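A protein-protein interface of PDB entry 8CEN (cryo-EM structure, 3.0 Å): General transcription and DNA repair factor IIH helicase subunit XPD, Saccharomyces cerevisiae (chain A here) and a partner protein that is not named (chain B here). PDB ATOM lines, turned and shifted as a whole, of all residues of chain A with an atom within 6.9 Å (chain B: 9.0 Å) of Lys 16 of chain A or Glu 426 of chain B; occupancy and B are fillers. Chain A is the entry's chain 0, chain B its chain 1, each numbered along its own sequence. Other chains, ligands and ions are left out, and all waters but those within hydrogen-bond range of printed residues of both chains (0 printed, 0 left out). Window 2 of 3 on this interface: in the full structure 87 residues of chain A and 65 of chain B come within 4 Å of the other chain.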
ATOM      1  N   MET A   1      -0.044 -22.257   7.894  1.00  0.00           N
ATOM      2  CA  MET A   1      -1.069 -21.738   7.000  1.00  0.00           C
ATOM      3  C   MET A   1      -1.708 -22.853   6.183  1.00  0.00           C
ATOM      4  O   MET A   1      -1.380 -24.029   6.344  1.00  0.00           O
ATOM      5  CB  MET A   1      -0.477 -20.691   6.063  1.00  0.00           C
ATOM      6  CG  MET A   1       0.544 -21.257   5.100  1.00  0.00           C
ATOM      7  SD  MET A   1       1.256 -19.989   4.046  1.00  0.00           S
ATOM      8  CE  MET A   1       2.386 -20.973   3.082  1.00  0.00           C
ATOM      9  N   PHE A  12       0.226 -26.403   5.827  1.00  0.00           N
ATOM     10  CA  PHE A  12       1.625 -26.317   6.232  1.00  0.00           C
ATOM     11  C   PHE A  12       1.708 -25.899   7.696  1.00  0.00           C
ATOM     12  O   PHE A  12       1.118 -24.882   8.072  1.00  0.00           O
ATOM     13  CB  PHE A  12       2.371 -25.314   5.364  1.00  0.00           C
ATOM     14  CG  PHE A  12       3.864 -25.454   5.417  1.00  0.00           C
ATOM     15  CD1 PHE A  12       4.471 -26.659   5.109  1.00  0.00           C
ATOM     16  CD2 PHE A  12       4.661 -24.378   5.771  1.00  0.00           C
ATOM     17  CE1 PHE A  12       5.845 -26.791   5.155  1.00  0.00           C
ATOM     18  CE2 PHE A  12       6.036 -24.505   5.820  1.00  0.00           C
ATOM     19  CZ  PHE A  12       6.627 -25.713   5.512  1.00  0.00           C
ATOM     20  N   PRO A  13       2.431 -26.628   8.547  1.00  0.00           N
ATOM     21  CA  PRO A  13       2.446 -26.313   9.981  1.00  0.00           C
ATOM     22  C   PRO A  13       3.281 -25.103  10.368  1.00  0.00           C
ATOM     23  O   PRO A  13       3.552 -24.921  11.557  1.00  0.00           O
ATOM     24  CB  PRO A  13       3.030 -27.592  10.601  1.00  0.00           C
ATOM     25  CG  PRO A  13       3.877 -28.156   9.546  1.00  0.00           C
ATOM     26  CD  PRO A  13       3.211 -27.837   8.241  1.00  0.00           C
ATOM     27  N   TYR A  14       3.693 -24.277   9.414  1.00  0.00           N
ATOM     28  CA  TYR A  14       4.406 -23.045   9.689  1.00  0.00           C
ATOM     29  C   TYR A  14       3.671 -21.888   9.033  1.00  0.00           C
ATOM     30  O   TYR A  14       3.078 -22.052   7.963  1.00  0.00           O
ATOM     31  CB  TYR A  14       5.846 -23.110   9.158  1.00  0.00           C
ATOM     32  CG  TYR A  14       6.710 -24.126   9.866  1.00  0.00           C
ATOM     33  CD1 TYR A  14       7.220 -23.872  11.131  1.00  0.00           C
ATOM     34  CD2 TYR A  14       7.014 -25.342   9.267  1.00  0.00           C
ATOM     35  CE1 TYR A  14       8.011 -24.801  11.781  1.00  0.00           C
ATOM     36  CE2 TYR A  14       7.803 -26.275   9.907  1.00  0.00           C
ATOM     37  CZ  TYR A  14       8.300 -26.000  11.163  1.00  0.00           C
ATOM     38  OH  TYR A  14       9.087 -26.928  11.804  1.00  0.00           O
ATOM     39  N   PRO A  15       3.675 -20.708   9.663  1.00  0.00           N
ATOM     40  CA  PRO A  15       3.055 -19.535   9.025  1.00  0.00           C
ATOM     41  C   PRO A  15       3.767 -19.080   7.764  1.00  0.00           C
ATOM     42  O   PRO A  15       3.151 -18.394   6.940  1.00  0.00           O
ATOM     43  CB  PRO A  15       3.123 -18.463  10.121  1.00  0.00           C
ATOM     44  CG  PRO A  15       4.250 -18.899  10.996  1.00  0.00           C
ATOM     45  CD  PRO A  15       4.203 -20.393  11.001  1.00  0.00           C
ATOM     46  N   LYS A  16       5.035 -19.439   7.587  1.00  0.00           N
ATOM     47  CA  LYS A  16       5.810 -19.061   6.417  1.00  0.00           C
ATOM     48  C   LYS A  16       6.355 -20.307   5.733  1.00  0.00           C
ATOM     49  O   LYS A  16       6.557 -21.345   6.369  1.00  0.00           O
ATOM     50  CB  LYS A  16       6.959 -18.127   6.800  1.00  0.00           C
ATOM     51  CG  LYS A  16       6.516 -16.743   7.238  1.00  0.00           C
ATOM     52  CD  LYS A  16       7.685 -15.776   7.263  1.00  0.00           C
ATOM     53  CE  LYS A  16       8.675 -16.144   8.354  1.00  0.00           C
ATOM     54  NZ  LYS A  16       8.092 -15.944   9.708  1.00  0.00           N
ATOM     55  N   ILE A  17       6.588 -20.197   4.424  1.00  0.00           N
ATOM     56  CA  ILE A  17       7.061 -21.311   3.616  1.00  0.00           C
ATOM     57  C   ILE A  17       8.259 -20.832   2.804  1.00  0.00           C
ATOM     58  O   ILE A  17       8.459 -19.635   2.591  1.00  0.00           O
ATOM     59  CB  ILE A  17       5.943 -21.866   2.694  1.00  0.00           C
ATOM     60  CG1 ILE A  17       6.246 -23.293   2.223  1.00  0.00           C
ATOM     61  CG2 ILE A  17       5.722 -20.953   1.494  1.00  0.00           C
ATOM     62  CD1 ILE A  17       5.185 -23.877   1.317  1.00  0.00           C
ATOM     63  N   TYR A  18       9.091 -21.794   2.381  1.00  0.00           N
ATOM     64  CA  TYR A  18      10.174 -21.490   1.463  1.00  0.00           C
ATOM     65  C   TYR A  18       9.733 -21.728   0.019  1.00  0.00           C
ATOM     66  O   TYR A  18       8.887 -22.596  -0.246  1.00  0.00           O
ATOM     67  CB  TYR A  18      11.395 -22.353   1.773  1.00  0.00           C
ATOM     68  CG  TYR A  18      12.060 -22.049   3.097  1.00  0.00           C
ATOM     69  CD1 TYR A  18      12.276 -20.742   3.506  1.00  0.00           C
ATOM     70  CD2 TYR A  18      12.488 -23.074   3.929  1.00  0.00           C
ATOM     71  CE1 TYR A  18      12.888 -20.462   4.714  1.00  0.00           C
ATOM     72  CE2 TYR A  18      13.102 -22.807   5.137  1.00  0.00           C
ATOM     73  CZ  TYR A  18      13.300 -21.500   5.524  1.00  0.00           C
ATOM     74  OH  TYR A  18      13.910 -21.228   6.726  1.00  0.00           O
ATOM     75  N   GLN A  21      10.454 -25.194  -0.822  1.00  0.00           N
ATOM     76  CA  GLN A  21       9.413 -26.071  -0.291  1.00  0.00           C
ATOM     77  C   GLN A  21       8.184 -26.093  -1.190  1.00  0.00           C
ATOM     78  O   GLN A  21       7.614 -27.161  -1.438  1.00  0.00           O
ATOM     79  CB  GLN A  21       9.018 -25.639   1.120  1.00  0.00           C
ATOM     80  CG  GLN A  21      10.119 -25.747   2.150  1.00  0.00           C
ATOM     81  CD  GLN A  21       9.663 -25.290   3.519  1.00  0.00           C
ATOM     82  OE1 GLN A  21       9.242 -24.148   3.695  1.00  0.00           O
ATOM     83  NE2 GLN A  21       9.736 -26.182   4.495  1.00  0.00           N
ATOM     84  N   GLN A 733      14.924 -10.158   3.390  1.00  0.00           N
ATOM     85  CA  GLN A 733      14.452 -11.540   3.350  1.00  0.00           C
ATOM     86  C   GLN A 733      12.930 -11.643   3.421  1.00  0.00           C
ATOM     87  O   GLN A 733      12.402 -12.706   3.765  1.00  0.00           O
ATOM     88  CB  GLN A 733      15.094 -12.357   4.474  1.00  0.00           C
ATOM     89  CG  GLN A 733      14.710 -11.923   5.880  1.00  0.00           C
ATOM     90  CD  GLN A 733      15.421 -12.727   6.949  1.00  0.00           C
ATOM     91  OE1 GLN A 733      16.174 -13.652   6.649  1.00  0.00           O
ATOM     92  NE2 GLN A 733      15.182 -12.378   8.208  1.00  0.00           N
ATOM     93  N   GLU A 734      12.216 -10.564   3.092  1.00  0.00           N
ATOM     94  CA  GLU A 734      10.763 -10.546   3.249  1.00  0.00           C
ATOM     95  C   GLU A 734      10.071 -11.466   2.249  1.00  0.00           C
ATOM     96  O   GLU A 734       9.174 -12.233   2.618  1.00  0.00           O
ATOM     97  CB  GLU A 734      10.243  -9.114   3.112  1.00  0.00           C
ATOM     98  CG  GLU A 734       8.735  -8.962   3.291  1.00  0.00           C
ATOM     99  CD  GLU A 734       8.263  -9.283   4.701  1.00  0.00           C
ATOM    100  OE1 GLU A 734       9.061  -9.140   5.653  1.00  0.00           O
ATOM    101  OE2 GLU A 734       7.090  -9.682   4.856  1.00  0.00           O
ATOM    102  N   VAL A 738      12.015 -16.427   1.944  1.00  0.00           N
ATOM    103  CA  VAL A 738      10.936 -17.088   2.667  1.00  0.00           C
ATOM    104  C   VAL A 738       9.630 -16.379   2.325  1.00  0.00           C
ATOM    105  O   VAL A 738       9.575 -15.146   2.263  1.00  0.00           O
ATOM    106  CB  VAL A 738      11.221 -17.119   4.190  1.00  0.00           C
ATOM    107  CG1 VAL A 738      11.514 -15.728   4.738  1.00  0.00           C
ATOM    108  CG2 VAL A 738      10.087 -17.780   4.949  1.00  0.00           C
ATOM    109  N   TRP A 739       8.587 -17.161   2.060  1.00  0.00           N
ATOM    110  CA  TRP A 739       7.310 -16.637   1.595  1.00  0.00           C
ATOM    111  C   TRP A 739       6.274 -16.656   2.708  1.00  0.00           C
ATOM    112  O   TRP A 739       6.204 -17.606   3.492  1.00  0.00           O
ATOM    113  CB  TRP A 739       6.777 -17.452   0.417  1.00  0.00           C
ATOM    114  CG  TRP A 739       7.428 -17.162  -0.884  1.00  0.00           C
ATOM    115  CD1 TRP A 739       8.181 -16.072  -1.202  1.00  0.00           C
ATOM    116  CD2 TRP A 739       7.383 -17.977  -2.056  1.00  0.00           C
ATOM    117  NE1 TRP A 739       8.610 -16.160  -2.504  1.00  0.00           N
ATOM    118  CE2 TRP A 739       8.132 -17.321  -3.050  1.00  0.00           C
ATOM    119  CE3 TRP A 739       6.782 -19.201  -2.360  1.00  0.00           C
ATOM    120  CZ2 TRP A 739       8.296 -17.848  -4.326  1.00  0.00           C
ATOM    121  CZ3 TRP A 739       6.945 -19.722  -3.625  1.00  0.00           C
ATOM    122  CH2 TRP A 739       7.701 -19.050  -4.591  1.00  0.00           C
ATOM    123  N   SER A 740       5.465 -15.603   2.767  1.00  0.00           N
ATOM    124  CA  SER A 740       4.248 -15.617   3.557  1.00  0.00           C
ATOM    125  C   SER A 740       3.109 -16.175   2.704  1.00  0.00           C
ATOM    126  O   SER A 740       3.303 -16.580   1.555  1.00  0.00           O
ATOM    127  CB  SER A 740       3.928 -14.217   4.075  1.00  0.00           C
ATOM    128  OG  SER A 740       2.729 -14.217   4.830  1.00  0.00           O
ATOM    129  N   TYR A 741       1.901 -16.204   3.276  1.00  0.00           N
ATOM    130  CA  TYR A 741       0.745 -16.689   2.529  1.00  0.00           C
ATOM    131  C   TYR A 741       0.411 -15.768   1.362  1.00  0.00           C
ATOM    132  O   TYR A 741       0.121 -16.239   0.257  1.00  0.00           O
ATOM    133  CB  TYR A 741      -0.464 -16.837   3.451  1.00  0.00           C
ATOM    134  CG  TYR A 741      -1.727 -17.218   2.713  1.00  0.00           C
ATOM    135  CD1 TYR A 741      -1.792 -18.394   1.975  1.00  0.00           C
ATOM    136  CD2 TYR A 741      -2.848 -16.400   2.745  1.00  0.00           C
ATOM    137  CE1 TYR A 741      -2.941 -18.747   1.294  1.00  0.00           C
ATOM    138  CE2 TYR A 741      -4.004 -16.745   2.067  1.00  0.00           C
ATOM    139  CZ  TYR A 741      -4.043 -17.920   1.344  1.00  0.00           C
ATOM    140  OH  TYR A 741      -5.188 -18.269   0.667  1.00  0.00           O
ATOM    141  N   ILE B 421      11.501 -25.720  13.249  1.00  0.00           N
ATOM    142  CA  ILE B 421      12.264 -24.744  12.477  1.00  0.00           C
ATOM    143  C   ILE B 421      11.885 -23.354  12.976  1.00  0.00           C
ATOM    144  O   ILE B 421      10.765 -22.887  12.749  1.00  0.00           O
ATOM    145  CB  ILE B 421      12.003 -24.886  10.974  1.00  0.00           C
ATOM    146  CG1 ILE B 421      12.389 -26.284  10.488  1.00  0.00           C
ATOM    147  CG2 ILE B 421      12.766 -23.826  10.199  1.00  0.00           C
ATOM    148  CD1 ILE B 421      11.957 -26.574   9.067  1.00  0.00           C
ATOM    149  N   ASP B 422      12.821 -22.690  13.657  1.00  0.00           N
ATOM    150  CA  ASP B 422      12.547 -21.369  14.210  1.00  0.00           C
ATOM    151  C   ASP B 422      12.489 -20.286  13.142  1.00  0.00           C
ATOM    152  O   ASP B 422      11.872 -19.241  13.372  1.00  0.00           O
ATOM    153  CB  ASP B 422      13.604 -21.007  15.254  1.00  0.00           C
ATOM    154  CG  ASP B 422      13.502 -21.856  16.507  1.00  0.00           C
ATOM    155  OD1 ASP B 422      12.384 -22.302  16.839  1.00  0.00           O
ATOM    156  OD2 ASP B 422      14.544 -22.080  17.158  1.00  0.00           O
ATOM    157  N   ASP B 423      13.119 -20.506  11.985  1.00  0.00           N
ATOM    158  CA  ASP B 423      13.099 -19.500  10.928  1.00  0.00           C
ATOM    159  C   ASP B 423      11.738 -19.417  10.251  1.00  0.00           C
ATOM    160  O   ASP B 423      11.312 -18.327   9.853  1.00  0.00           O
ATOM    161  CB  ASP B 423      14.188 -19.801   9.898  1.00  0.00           C
ATOM    162  CG  ASP B 423      14.271 -18.744   8.813  1.00  0.00           C
ATOM    163  OD1 ASP B 423      14.649 -17.596   9.127  1.00  0.00           O
ATOM    164  OD2 ASP B 423      13.959 -19.062   7.646  1.00  0.00           O
ATOM    165  N   LEU B 424      11.044 -20.545  10.112  1.00  0.00           N
ATOM    166  CA  LEU B 424       9.747 -20.568   9.448  1.00  0.00           C
ATOM    167  C   LEU B 424       8.608 -20.094  10.342  1.00  0.00           C
ATOM    168  O   LEU B 424       7.508 -19.852   9.835  1.00  0.00           O
ATOM    169  CB  LEU B 424       9.445 -21.978   8.937  1.00  0.00           C
ATOM    170  CG  LEU B 424      10.077 -22.368   7.600  1.00  0.00           C
ATOM    171  CD1 LEU B 424       9.496 -23.677   7.094  1.00  0.00           C
ATOM    172  CD2 LEU B 424       9.882 -21.265   6.575  1.00  0.00           C
ATOM    173  N   ASN B 425       8.841 -19.957  11.645  1.00  0.00           N
ATOM    174  CA  ASN B 425       7.817 -19.468  12.554  1.00  0.00           C
ATOM    175  C   ASN B 425       7.691 -17.951  12.439  1.00  0.00           C
ATOM    176  O   ASN B 425       8.420 -17.292  11.691  1.00  0.00           O
ATOM    177  CB  ASN B 425       8.139 -19.884  13.988  1.00  0.00           C
ATOM    178  CG  ASN B 425       7.808 -21.337  14.261  1.00  0.00           C
ATOM    179  OD1 ASN B 425       6.845 -21.878  13.719  1.00  0.00           O
ATOM    180  ND2 ASN B 425       8.605 -21.976  15.109  1.00  0.00           N
ATOM    181  N   GLU B 426       6.743 -17.389  13.184  1.00  0.00           N
ATOM    182  CA  GLU B 426       6.558 -15.946  13.203  1.00  0.00           C
ATOM    183  C   GLU B 426       7.742 -15.256  13.869  1.00  0.00           C
ATOM    184  O   GLU B 426       8.357 -15.786  14.798  1.00  0.00           O
ATOM    185  CB  GLU B 426       5.266 -15.575  13.938  1.00  0.00           C
ATOM    186  CG  GLU B 426       3.982 -16.022  13.251  1.00  0.00           C
ATOM    187  CD  GLU B 426       3.453 -15.010  12.245  1.00  0.00           C
ATOM    188  OE1 GLU B 426       4.260 -14.341  11.566  1.00  0.00           O
ATOM    189  OE2 GLU B 426       2.216 -14.883  12.133  1.00  0.00           O
ATOM    190  N   SER B 427       8.064 -14.065  13.373  1.00  0.00           N
ATOM    191  CA  SER B 427       9.105 -13.253  13.983  1.00  0.00           C
ATOM    192  C   SER B 427       8.664 -12.786  15.364  1.00  0.00           C
ATOM    193  O   SER B 427       7.470 -12.676  15.656  1.00  0.00           O
ATOM    194  CB  SER B 427       9.433 -12.050  13.098  1.00  0.00           C
ATOM    195  OG  SER B 427       8.286 -11.245  12.889  1.00  0.00           O
ATOM    196  N   TYR B 428       9.647 -12.528  16.225  1.00  0.00           N
ATOM    197  CA  TYR B 428       9.359 -12.147  17.601  1.00  0.00           C
ATOM    198  C   TYR B 428       8.712 -10.768  17.648  1.00  0.00           C
ATOM    199  O   TYR B 428       9.206  -9.815  17.037  1.00  0.00           O
ATOM    200  CB  TYR B 428      10.639 -12.160  18.436  1.00  0.00           C
ATOM    201  CG  TYR B 428      10.502 -11.448  19.763  1.00  0.00           C
ATOM    202  CD1 TYR B 428       9.760 -12.008  20.797  1.00  0.00           C
ATOM    203  CD2 TYR B 428      11.116 -10.221  19.986  1.00  0.00           C
ATOM    204  CE1 TYR B 428       9.629 -11.364  22.012  1.00  0.00           C
ATOM    205  CE2 TYR B 428      10.988  -9.569  21.198  1.00  0.00           C
ATOM    206  CZ  TYR B 428      10.245 -10.146  22.207  1.00  0.00           C
ATOM    207  OH  TYR B 428      10.118  -9.502  23.417  1.00  0.00           O
ATOM    208  N   LYS B 429       7.606 -10.668  18.377  1.00  0.00           N
ATOM    209  CA  LYS B 429       6.871  -9.420  18.529  1.00  0.00           C
ATOM    210  C   LYS B 429       7.227  -8.826  19.886  1.00  0.00           C
ATOM    211  O   LYS B 429       7.050  -9.480  20.920  1.00  0.00           O
ATOM    212  CB  LYS B 429       5.365  -9.665  18.389  1.00  0.00           C
ATOM    213  CG  LYS B 429       4.448  -8.437  18.503  1.00  0.00           C
ATOM    214  CD  LYS B 429       3.911  -8.204  19.914  1.00  0.00           C
ATOM    215  CE  LYS B 429       2.896  -9.265  20.304  1.00  0.00           C
ATOM    216  NZ  LYS B 429       2.359  -9.038  21.674  1.00  0.00           N
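OH of Tyr 14 of chain A is in hydrogen-bond range of N of Ile 421 of chain B, at 3.1 Å.
N of Lys 16 of chain A is in hydrogen-bond range of O of Leu 424 of chain B.
The side-chain amino group of Lys 16 of chain A lies within hydrogen-bond range of the backbone carbonyl oxygen of Asn 425 of chain B (2.4 Å).
OH of Tyr 18 of chain A sits close to OD2 of Asp 423 of chain B (2.4 Å).
N of Met 1 of chain A lies within hydrogen-bond range of O of Phe 12 of chain A (2.9 Å).
O of Tyr 14 of chain A sits at hydrogen-bond distance from N of Met 1 of chain A, 3.1 Å away.
The backbone NH (N) of Tyr 18 of chain A lies within hydrogen-bond range of the side-chain amide oxygen (OE1) of Gln 21 of chain A, 2.7 Å away.
ND2 of Asn 425 of chain B lies within hydrogen-bond range of O of Ile 421 of chain B (3.3 Å).
Among the printed residues, merely in contact across the chains: Phe 12 of chain A with Leu 424 of chain B (3.8 Å), Tyr 14 of chain A with Leu 424 of chain B (3.6 Å), Tyr 14 of chain A with Asn 425 of chain B (3.3 Å), Pro 15 of chain A with Leu 424 of chain B (3.5 Å), Pro 15 of chain A with Asn 425 of chain B (3.8 Å), Pro 15 of chain A with Glu 426 of chain B (3.6 Å), Lys 16 of chain A with Asp 423 of chain B (3.7 Å), Lys 16 of chain A with Glu 426 of chain B (3.8 Å), Tyr 18 of chain A with Leu 424 of chain B (3.6 Å), Gln 21 of chain A with Leu 424 of chain B (3.4 Å) and Val 738 of chain A with Leu 424 of chain B (3.9 Å).
Lys 16 of chain A touches four residues of chain B.
Glu 426 of chain B touches just these residues of chain A: Pro 15 and Lys 16.
Of the printed residues of chain A, Leu 424 of chain B touches Phe 12, Tyr 14, Pro 15, Lys 16, Tyr 18, Gln 21 and Val 738.
Of the printed residues of chain B, Phe 12 of chain A touches Leu 424.
Printed residues of chain B within 4 Å of Tyr 14 of chain A: Ile 421 (3.1 Å), Leu 424 (3.6 Å) and Asn 425 (3.3 Å).
Printed residues of chain B within 4 Å of Tyr 18 of chain A: Asp 423 (2.4 Å) and Leu 424 (3.6 Å).
Glu 734 of chain A touches none of the printed residues of chain B.
Gln 733 of chain A touches none of the printed residues of chain B.
The nearest residue of chain A that does not touch Glu 426 of chain B is Tyr 14 of chain A (6.8 Å).
Of the 9 printed residues of chain B, 5 touch a printed residue of chain A.
Hydrophobic or aromatic side chains of chain B that line the printed part of chain A: Ile 421 and Leu 424.
Printed residues of chain A that touch a printed residue of chain B: Phe 12, Tyr 14, Pro 15, Lys 16, Tyr 18, Gln 21 and Val 738.
Hydrophobic or aromatic side chains of chain A within 4 Å of the printed part of chain B: Phe 12, Tyr 14, Pro 15, Tyr 18 and Val 738.
Among the printed residues, 15 pairs touch across the chains.
Among the printed residues, no Asp or Glu carboxylate lies within 4 Å of a Lys or Arg side-chain nitrogen of the other chain.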
